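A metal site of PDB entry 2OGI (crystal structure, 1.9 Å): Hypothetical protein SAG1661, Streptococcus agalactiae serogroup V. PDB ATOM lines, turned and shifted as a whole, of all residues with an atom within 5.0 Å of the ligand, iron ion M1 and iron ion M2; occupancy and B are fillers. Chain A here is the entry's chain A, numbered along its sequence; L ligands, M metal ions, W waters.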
ATOM      1  N   HIS A  30     -32.304  14.267   4.480  1.00  0.00           N
ATOM      2  CA  HIS A  30     -31.156  15.126   4.550  1.00  0.00           C
ATOM      3  C   HIS A  30     -30.701  15.267   5.977  1.00  0.00           C
ATOM      4  O   HIS A  30     -29.518  15.175   6.290  1.00  0.00           O
ATOM      5  CB  HIS A  30     -31.472  16.474   3.955  1.00  0.00           C
ATOM      6  CG  HIS A  30     -30.548  17.569   4.391  1.00  0.00           C
ATOM      7  ND1 HIS A  30     -29.254  17.629   3.961  1.00  0.00           N
ATOM      8  CD2 HIS A  30     -30.744  18.637   5.189  1.00  0.00           C
ATOM      9  CE1 HIS A  30     -28.672  18.711   4.482  1.00  0.00           C
ATOM     10  NE2 HIS A  30     -29.578  19.360   5.198  1.00  0.00           N
ATOM     11  N   VAL A  34     -27.196  14.372   7.609  1.00  0.00           N
ATOM     12  CA  VAL A  34     -26.380  15.287   8.376  1.00  0.00           C
ATOM     13  C   VAL A  34     -26.048  14.766   9.771  1.00  0.00           C
ATOM     14  O   VAL A  34     -24.936  14.930  10.255  1.00  0.00           O
ATOM     15  CB  VAL A  34     -27.035  16.700   8.464  1.00  0.00           C
ATOM     16  CG1 VAL A  34     -26.141  17.649   9.290  1.00  0.00           C
ATOM     17  CG2 VAL A  34     -27.202  17.272   7.081  1.00  0.00           C
ATOM     18  N   HIS A  59     -30.834  20.853  13.043  1.00  0.00           N
ATOM     19  CA  HIS A  59     -30.313  22.102  12.423  1.00  0.00           C
ATOM     20  C   HIS A  59     -31.301  22.764  11.468  1.00  0.00           C
ATOM     21  O   HIS A  59     -31.378  23.969  11.403  1.00  0.00           O
ATOM     22  CB  HIS A  59     -28.934  21.866  11.779  1.00  0.00           C
ATOM     23  CG  HIS A  59     -29.002  21.251  10.447  1.00  0.00           C
ATOM     24  ND1 HIS A  59     -29.302  19.925  10.247  1.00  0.00           N
ATOM     25  CD2 HIS A  59     -28.904  21.796   9.222  1.00  0.00           C
ATOM     26  CE1 HIS A  59     -29.362  19.681   8.949  1.00  0.00           C
ATOM     27  NE2 HIS A  59     -29.148  20.808   8.299  1.00  0.00           N
ATOM     28  N   ASP A  60     -32.064  21.951  10.755  1.00  0.00           N
ATOM     29  CA  ASP A  60     -33.076  22.380   9.798  1.00  0.00           C
ATOM     30  C   ASP A  60     -34.482  22.205  10.321  1.00  0.00           C
ATOM     31  O   ASP A  60     -35.377  22.063   9.566  1.00  0.00           O
ATOM     32  CB  ASP A  60     -32.894  21.590   8.500  1.00  0.00           C
ATOM     33  CG  ASP A  60     -31.929  22.306   7.514  1.00  0.00           C
ATOM     34  OD1 ASP A  60     -31.590  23.510   7.739  1.00  0.00           O
ATOM     35  OD2 ASP A  60     -31.492  21.655   6.536  1.00  0.00           O
ATOM     36  N   LYS A  63     -36.769  24.710   8.660  1.00  0.00           N
ATOM     37  CA  LYS A  63     -36.518  24.949   7.257  1.00  0.00           C
ATOM     38  C   LYS A  63     -37.788  25.263   6.463  1.00  0.00           C
ATOM     39  O   LYS A  63     -37.746  26.049   5.543  1.00  0.00           O
ATOM     40  CB  LYS A  63     -35.816  23.736   6.653  1.00  0.00           C
ATOM     41  CG  LYS A  63     -35.400  23.812   5.190  1.00  0.00           C
ATOM     42  CD  LYS A  63     -34.411  24.912   4.834  1.00  0.00           C
ATOM     43  CE  LYS A  63     -33.836  24.603   3.467  1.00  0.00           C
ATOM     44  NZ  LYS A  63     -32.967  25.628   2.873  1.00  0.00           N
ATOM     45  N   TRP A  86     -34.380  39.810   4.516  1.00  0.00           N
ATOM     46  CA  TRP A  86     -33.784  38.627   3.975  1.00  0.00           C
ATOM     47  C   TRP A  86     -34.900  37.607   3.765  1.00  0.00           C
ATOM     48  O   TRP A  86     -36.017  37.954   3.370  1.00  0.00           O
ATOM     49  CB  TRP A  86     -32.618  38.143   4.833  1.00  0.00           C
ATOM     50  CG  TRP A  86     -31.509  39.136   4.871  1.00  0.00           C
ATOM     51  CD1 TRP A  86     -31.411  40.191   5.689  1.00  0.00           C
ATOM     52  CD2 TRP A  86     -30.369  39.189   4.014  1.00  0.00           C
ATOM     53  NE1 TRP A  86     -30.262  40.906   5.428  1.00  0.00           N
ATOM     54  CE2 TRP A  86     -29.601  40.303   4.405  1.00  0.00           C
ATOM     55  CE3 TRP A  86     -29.884  38.361   2.988  1.00  0.00           C
ATOM     56  CZ2 TRP A  86     -28.396  40.653   3.772  1.00  0.00           C
ATOM     57  CZ3 TRP A  86     -28.674  38.716   2.348  1.00  0.00           C
ATOM     58  CH2 TRP A  86     -27.958  39.852   2.739  1.00  0.00           C
ATOM     59  N   ASN A  89     -33.538  31.444   3.776  1.00  0.00           N
ATOM     60  CA  ASN A  89     -32.182  30.924   3.787  1.00  0.00           C
ATOM     61  C   ASN A  89     -31.479  31.413   5.039  1.00  0.00           C
ATOM     62  O   ASN A  89     -30.745  30.699   5.748  1.00  0.00           O
ATOM     63  CB  ASN A  89     -31.371  31.401   2.557  1.00  0.00           C
ATOM     64  CG  ASN A  89     -31.718  30.682   1.288  1.00  0.00           C
ATOM     65  OD1 ASN A  89     -32.481  29.702   1.283  1.00  0.00           O
ATOM     66  ND2 ASN A  89     -31.194  31.200   0.168  1.00  0.00           N
ATOM     67  N   ILE A  90     -31.721  32.672   5.341  1.00  0.00           N
ATOM     68  CA  ILE A  90     -31.073  33.310   6.471  1.00  0.00           C
ATOM     69  C   ILE A  90     -31.852  33.009   7.743  1.00  0.00           C
ATOM     70  O   ILE A  90     -31.273  32.813   8.800  1.00  0.00           O
ATOM     71  CB  ILE A  90     -31.000  34.862   6.237  1.00  0.00           C
ATOM     72  CG1 ILE A  90     -30.063  35.219   5.075  1.00  0.00           C
ATOM     73  CG2 ILE A  90     -30.577  35.602   7.465  1.00  0.00           C
ATOM     74  CD1 ILE A  90     -28.883  34.377   4.959  1.00  0.00           C
ATOM     75  N   HIS A  92     -33.978  30.489   8.660  1.00  0.00           N
ATOM     76  CA  HIS A  92     -34.351  29.190   9.253  1.00  0.00           C
ATOM     77  C   HIS A  92     -33.432  28.712  10.333  1.00  0.00           C
ATOM     78  O   HIS A  92     -33.906  27.936  11.176  1.00  0.00           O
ATOM     79  CB  HIS A  92     -34.641  28.107   8.184  1.00  0.00           C
ATOM     80  CG  HIS A  92     -33.410  27.568   7.505  1.00  0.00           C
ATOM     81  ND1 HIS A  92     -32.796  28.242   6.478  1.00  0.00           N
ATOM     82  CD2 HIS A  92     -32.647  26.470   7.762  1.00  0.00           C
ATOM     83  CE1 HIS A  92     -31.715  27.556   6.089  1.00  0.00           C
ATOM     84  NE2 HIS A  92     -31.604  26.488   6.860  1.00  0.00           N
ATOM     85  N   HIS A 118     -25.624  27.767  11.239  1.00  0.00           N
ATOM     86  CA  HIS A 118     -25.309  26.667  10.328  1.00  0.00           C
ATOM     87  C   HIS A 118     -25.259  27.067   8.864  1.00  0.00           C
ATOM     88  O   HIS A 118     -24.555  26.427   8.117  1.00  0.00           O
ATOM     89  CB  HIS A 118     -26.233  25.444  10.525  1.00  0.00           C
ATOM     90  CG  HIS A 118     -27.541  25.513   9.799  1.00  0.00           C
ATOM     91  ND1 HIS A 118     -28.697  25.959  10.405  1.00  0.00           N
ATOM     92  CD2 HIS A 118     -27.928  25.052   8.581  1.00  0.00           C
ATOM     93  CE1 HIS A 118     -29.711  25.827   9.570  1.00  0.00           C
ATOM     94  NE2 HIS A 118     -29.282  25.274   8.461  1.00  0.00           N
ATOM     95  N   THR A 119     -25.965  28.110   8.458  1.00  0.00           N
ATOM     96  CA  THR A 119     -26.026  28.499   7.055  1.00  0.00           C
ATOM     97  C   THR A 119     -24.899  29.477   6.733  1.00  0.00           C
ATOM     98  O   THR A 119     -24.223  29.351   5.749  1.00  0.00           O
ATOM     99  CB  THR A 119     -27.409  29.133   6.702  1.00  0.00           C
ATOM    100  OG1 THR A 119     -28.454  28.315   7.229  1.00  0.00           O
ATOM    101  CG2 THR A 119     -27.560  29.355   5.186  1.00  0.00           C
ATOM    102  N   VAL A 120     -24.630  30.435   7.613  1.00  0.00           N
ATOM    103  CA  VAL A 120     -23.733  31.538   7.312  1.00  0.00           C
ATOM    104  C   VAL A 120     -22.374  31.497   8.012  1.00  0.00           C
ATOM    105  O   VAL A 120     -21.434  32.155   7.583  1.00  0.00           O
ATOM    106  CB  VAL A 120     -24.441  32.867   7.638  1.00  0.00           C
ATOM    107  CG1 VAL A 120     -25.638  32.987   6.745  1.00  0.00           C
ATOM    108  CG2 VAL A 120     -24.896  32.939   9.034  1.00  0.00           C
ATOM    109  N   ASP A 136     -23.522  19.428   7.074  1.00  0.00           N
ATOM    110  CA  ASP A 136     -24.670  19.863   6.257  1.00  0.00           C
ATOM    111  C   ASP A 136     -24.388  19.836   4.760  1.00  0.00           C
ATOM    112  O   ASP A 136     -25.269  19.541   3.943  1.00  0.00           O
ATOM    113  CB  ASP A 136     -25.048  21.292   6.690  1.00  0.00           C
ATOM    114  CG  ASP A 136     -26.368  21.752   6.098  1.00  0.00           C
ATOM    115  OD1 ASP A 136     -27.277  20.891   5.905  1.00  0.00           O
ATOM    116  OD2 ASP A 136     -26.464  22.949   5.764  1.00  0.00           O
ATOM    117  N   ARG A 142     -26.265  14.468  -0.575  1.00  0.00           N
ATOM    118  CA  ARG A 142     -25.864  15.617  -1.405  1.00  0.00           C
ATOM    119  C   ARG A 142     -25.096  15.177  -2.654  1.00  0.00           C
ATOM    120  O   ARG A 142     -24.291  14.267  -2.588  1.00  0.00           O
ATOM    121  CB  ARG A 142     -24.970  16.605  -0.656  1.00  0.00           C
ATOM    122  CG  ARG A 142     -25.550  17.266   0.576  1.00  0.00           C
ATOM    123  CD  ARG A 142     -26.549  18.348   0.258  1.00  0.00           C
ATOM    124  NE  ARG A 142     -26.436  19.410   1.252  1.00  0.00           N
ATOM    125  CZ  ARG A 142     -27.418  20.223   1.633  1.00  0.00           C
ATOM    126  NH1 ARG A 142     -28.635  20.104   1.121  1.00  0.00           N
ATOM    127  NH2 ARG A 142     -27.190  21.161   2.568  1.00  0.00           N
ATOM    128  N   THR A 169     -19.806  28.710  -1.753  1.00  0.00           N
ATOM    129  CA  THR A 169     -21.121  29.271  -1.585  1.00  0.00           C
ATOM    130  C   THR A 169     -21.081  30.752  -2.042  1.00  0.00           C
ATOM    131  O   THR A 169     -21.973  31.215  -2.670  1.00  0.00           O
ATOM    132  CB  THR A 169     -21.570  29.157  -0.117  1.00  0.00           C
ATOM    133  OG1 THR A 169     -21.691  27.754   0.221  1.00  0.00           O
ATOM    134  CG2 THR A 169     -22.825  29.913   0.144  1.00  0.00           C
ATOM    135  N   PHE A 172     -21.036  30.821  -5.754  1.00  0.00           N
ATOM    136  CA  PHE A 172     -22.345  30.405  -6.292  1.00  0.00           C
ATOM    137  C   PHE A 172     -23.375  31.554  -6.254  1.00  0.00           C
ATOM    138  O   PHE A 172     -24.102  31.798  -7.212  1.00  0.00           O
ATOM    139  CB  PHE A 172     -22.841  29.195  -5.493  1.00  0.00           C
ATOM    140  CG  PHE A 172     -24.280  28.873  -5.712  1.00  0.00           C
ATOM    141  CD1 PHE A 172     -24.695  28.200  -6.832  1.00  0.00           C
ATOM    142  CD2 PHE A 172     -25.250  29.292  -4.807  1.00  0.00           C
ATOM    143  CE1 PHE A 172     -26.021  27.915  -7.047  1.00  0.00           C
ATOM    144  CE2 PHE A 172     -26.575  29.020  -5.029  1.00  0.00           C
ATOM    145  CZ  PHE A 172     -26.949  28.327  -6.142  1.00  0.00           C
ATOM    146  N   LEU A 173     -23.434  32.241  -5.127  1.00  0.00           N
ATOM    147  CA  LEU A 173     -24.378  33.327  -4.913  1.00  0.00           C
ATOM    148  C   LEU A 173     -24.063  34.488  -5.850  1.00  0.00           C
ATOM    149  O   LEU A 173     -24.951  35.104  -6.402  1.00  0.00           O
ATOM    150  CB  LEU A 173     -24.273  33.804  -3.451  1.00  0.00           C
ATOM    151  CG  LEU A 173     -24.802  32.841  -2.354  1.00  0.00           C
ATOM    152  CD1 LEU A 173     -24.456  33.392  -0.977  1.00  0.00           C
ATOM    153  CD2 LEU A 173     -26.288  32.632  -2.491  1.00  0.00           C
ATOM    154  N   GLN A 178     -27.218  37.052  -6.236  1.00  0.00           N
ATOM    155  CA  GLN A 178     -28.090  36.947  -5.057  1.00  0.00           C
ATOM    156  C   GLN A 178     -27.408  37.573  -3.892  1.00  0.00           C
ATOM    157  O   GLN A 178     -26.188  37.526  -3.782  1.00  0.00           O
ATOM    158  CB  GLN A 178     -28.337  35.484  -4.674  1.00  0.00           C
ATOM    159  CG  GLN A 178     -29.037  34.666  -5.733  1.00  0.00           C
ATOM    160  CD  GLN A 178     -30.382  35.201  -6.047  1.00  0.00           C
ATOM    161  OE1 GLN A 178     -31.183  35.460  -5.138  1.00  0.00           O
ATOM    162  NE2 GLN A 178     -30.662  35.394  -7.340  1.00  0.00           N
ATOM    163  N   PRO A 179     -28.199  38.155  -2.993  1.00  0.00           N
ATOM    164  CA  PRO A 179     -27.506  38.841  -1.896  1.00  0.00           C
ATOM    165  C   PRO A 179     -26.737  37.899  -1.032  1.00  0.00           C
ATOM    166  O   PRO A 179     -27.108  36.726  -0.896  1.00  0.00           O
ATOM    167  CB  PRO A 179     -28.630  39.573  -1.131  1.00  0.00           C
ATOM    168  CG  PRO A 179     -29.874  38.927  -1.549  1.00  0.00           C
ATOM    169  CD  PRO A 179     -29.667  38.246  -2.886  1.00  0.00           C
ATOM    170  N   ILE A 180     -25.648  38.436  -0.494  1.00  0.00           N
ATOM    171  CA  ILE A 180     -24.724  37.716   0.281  1.00  0.00           C
ATOM    172  C   ILE A 180     -24.774  38.341   1.668  1.00  0.00           C
ATOM    173  O   ILE A 180     -24.501  39.507   1.841  1.00  0.00           O
ATOM    174  CB  ILE A 180     -23.290  37.801  -0.336  1.00  0.00           C
ATOM    175  CG1 ILE A 180     -23.235  37.039  -1.650  1.00  0.00           C
ATOM    176  CG2 ILE A 180     -22.230  37.333   0.662  1.00  0.00           C
ATOM    177  CD1 ILE A 180     -21.996  37.332  -2.469  1.00  0.00           C
ATOM    178  N   TYR A 181     -25.185  37.522   2.638  1.00  0.00           N
ATOM    179  CA  TYR A 181     -25.307  37.927   4.009  1.00  0.00           C
ATOM    180  C   TYR A 181     -23.972  38.289   4.503  1.00  0.00           C
ATOM    181  O   TYR A 181     -23.015  37.619   4.226  1.00  0.00           O
ATOM    182  CB  TYR A 181     -25.942  36.836   4.901  1.00  0.00           C
ATOM    183  CG  TYR A 181     -26.488  37.306   6.254  1.00  0.00           C
ATOM    184  CD1 TYR A 181     -27.571  38.187   6.317  1.00  0.00           C
ATOM    185  CD2 TYR A 181     -25.930  36.863   7.450  1.00  0.00           C
ATOM    186  CE1 TYR A 181     -28.095  38.602   7.519  1.00  0.00           C
ATOM    187  CE2 TYR A 181     -26.459  37.261   8.680  1.00  0.00           C
ATOM    188  CZ  TYR A 181     -27.535  38.123   8.693  1.00  0.00           C
ATOM    189  OH  TYR A 181     -28.076  38.550   9.874  1.00  0.00           O
ATOM    190  N   THR A 184     -21.650  35.799   6.116  1.00  0.00           N
ATOM    191  CA  THR A 184     -21.087  34.866   5.172  1.00  0.00           C
ATOM    192  C   THR A 184     -19.676  35.307   4.743  1.00  0.00           C
ATOM    193  O   THR A 184     -18.791  34.489   4.629  1.00  0.00           O
ATOM    194  CB  THR A 184     -22.025  34.700   3.983  1.00  0.00           C
ATOM    195  OG1 THR A 184     -23.201  34.134   4.511  1.00  0.00           O
ATOM    196  CG2 THR A 184     -21.470  33.763   2.898  1.00  0.00           C
HETATM  197  P1  LIG L   1     -29.954  23.577   3.614  1.00  0.00           P
HETATM  198  O1  LIG L   1     -30.489  23.702   2.208  1.00  0.00           O
HETATM  199  O2  LIG L   1     -30.940  24.260   4.563  1.00  0.00           O
HETATM  200  O3  LIG L   1     -29.635  22.122   3.992  1.00  0.00           O
HETATM  201  O4  LIG L   1     -28.487  24.319   3.564  1.00  0.00           O
HETATM  202  P2  LIG L   1     -28.083  25.739   4.250  1.00  0.00           P
HETATM  203  O5  LIG L   1     -28.804  26.164   5.513  1.00  0.00           O
HETATM  204  O6  LIG L   1     -26.574  25.787   4.418  1.00  0.00           O
HETATM  205  O7  LIG L   1     -28.341  26.880   3.098  1.00  0.00           O
HETATM  206  C1  LIG L   1     -29.548  27.026   2.376  1.00  0.00           C
HETATM  207  C2  LIG L   1     -29.340  28.071   1.269  1.00  0.00           C
HETATM  208  O8  LIG L   1     -28.897  29.282   1.878  1.00  0.00           O
HETATM  209  C3  LIG L   1     -28.335  27.721   0.162  1.00  0.00           C
HETATM  210  O9  LIG L   1     -28.938  27.904  -1.129  1.00  0.00           O
HETATM  211  C4  LIG L   1     -27.205  28.716   0.307  1.00  0.00           C
HETATM  212  O10 LIG L   1     -26.663  29.137  -0.950  1.00  0.00           O
HETATM  213  C5  LIG L   1     -27.980  29.859   0.951  1.00  0.00           C
HETATM  214  N1  LIG L   1     -27.054  30.838   1.545  1.00  0.00           N
HETATM  215  C6  LIG L   1     -25.970  30.597   2.261  1.00  0.00           C
HETATM  216  N2  LIG L   1     -25.371  31.770   2.624  1.00  0.00           N
HETATM  217  C7  LIG L   1     -26.113  32.765   2.052  1.00  0.00           C
HETATM  218  C8  LIG L   1     -26.021  34.228   1.950  1.00  0.00           C
HETATM  219  O11 LIG L   1     -25.053  34.759   2.543  1.00  0.00           O
HETATM  220  N3  LIG L   1     -26.995  34.894   1.243  1.00  0.00           N
HETATM  221  C9  LIG L   1     -28.032  34.236   0.594  1.00  0.00           C
HETATM  222  N4  LIG L   1     -28.994  34.912  -0.140  1.00  0.00           N
HETATM  223  N5  LIG L   1     -28.145  32.872   0.658  1.00  0.00           N
HETATM  224  C10 LIG L   1     -27.237  32.141   1.354  1.00  0.00           C
HETATM  225 FE    FE M   1     -30.227  24.751   6.587  1.00  0.00          FE
HETATM  226 FE    FE M   2     -29.370  21.381   6.108  1.00  0.00          FE
HETATM  227  O   HOH W   1     -24.809  23.629   3.090  1.00  0.00           O
HETATM  228  O   HOH W   2     -23.235  30.792   3.685  1.00  0.00           O
HETATM  229  O   HOH W   3     -23.909  25.144   5.910  1.00  0.00           O
HETATM  230  O   HOH W   4     -30.295  33.354  -2.417  1.00  0.00           O
HETATM  231  O   HOH W   5     -28.868  23.252   6.401  1.00  0.00           O
HETATM  232  O   HOH W   6     -32.168  25.440  -0.071  1.00  0.00           O
HETATM  233  O   HOH W   7     -29.384  30.435  -3.078  1.00  0.00           O
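Of the 22 residues printed, 3 come within 4 Å of iron ion M1.
The nearest printed residue that does not touch iron ion M1 is Thr 119 (4.03 Å).
Iron ion M1 is bound by water W5 (2.0 Å), NE2 of His 118 (2.2 Å), OD1 of Asp 60 (2.2 Å), O2 of the ligand (2.2 Å), NE2 of His 92 (2.2 Å) and O5 of the ligand (2.3 Å).
Iron ion M1 has six donor atoms within binding distance.
An oxygen (O1) of the ligand is in salt-bridge range of the side-chain amino group (NZ) of Lys 63 (3.2 Å).
The backbone NH (N) of Tyr 181 lies within hydrogen-bond range of an oxygen (O11) of the ligand.
The backbone carbonyl oxygen (O) of Pro 179 sits at hydrogen-bond distance from a nitrogen (N4) of the ligand, 2.7 Å away.
The side-chain hydroxyl (OG1) of Thr 119 lies close to an oxygen (O5) of the ligand.
O11 of the ligand is in hydrogen-bond range of OG1 of Thr 184 (2.8 Å).
An oxygen (O8) of the ligand sits close to the side-chain amide nitrogen (ND2) of Asn 89 (3.4 Å).
NH2 of Arg 142 lies close to O3 of the ligand, at 3.0 Å.
Within 4 Å of iron ion M2: His 30, His 59, Asp 60 and Asp 136.
The nearest printed residue that does not touch iron ion M2 is Arg 142 (4.2 Å).
O of His 59 sits close to ND1 of His 118 (3.5 Å).
The backbone carbonyl oxygen of Leu 173 lies within hydrogen-bond range of the backbone NH of Gln 178 (3.0 Å).
NE2 of His 118 lies close to OG1 of Thr 119, 3.4 Å away.
A ring nitrogen (ND1) of His 92 is in hydrogen-bond range of the backbone carbonyl oxygen (O) of Asn 89, 3.3 Å away.
The side-chain carboxylate of Asp 136 lies within salt-bridge range of the guanidinium group of Arg 142 (3.7 Å).
Water W5 bridges OD2 of Asp 136 (2.5 Å) and O4 of the ligand (3.1 Å).
Water W2 lies within hydrogen-bond range of N2 of the ligand, O of Thr 119 and OG1 of Thr 184.
Water W4 bridges N4 of the ligand and ND2 of Asn 89.
Water W1 lies within hydrogen-bond range of an oxygen (O6) of the ligand (3.1 Å), the side-chain carboxylate (OD2) of Asp 136 (3.2 Å) and the guanidinium group (NH2) of Arg 142 (3.5 Å).
Water W3 lies within hydrogen-bond range of the backbone carbonyl oxygen (O) of His 118 (2.6 Å), an oxygen (O6) of the ligand (3.1 Å) and the side-chain carboxylate (OD2) of Asp 136 (3.4 Å).
Water W6 lies within hydrogen-bond range of NZ of Lys 63 (3.1 Å) and O1 of the ligand (3.3 Å).
Iron ion M2 is bound by water W5 (2.0 Å), the side-chain carboxylate (OD1) of Asp 136 (2.2 Å), the side-chain carboxylate (OD2) of Asp 60 (2.2 Å), a ring nitrogen (NE2) of His 30 (2.2 Å), an oxygen (O3) of the ligand (2.3 Å) and a ring nitrogen (NE2) of His 59 (2.3 Å).
Residues that only touch the ligand: Thr 169 (3.9 Å), Leu 173 (3.4 Å) and Ile 180 (3.7 Å).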
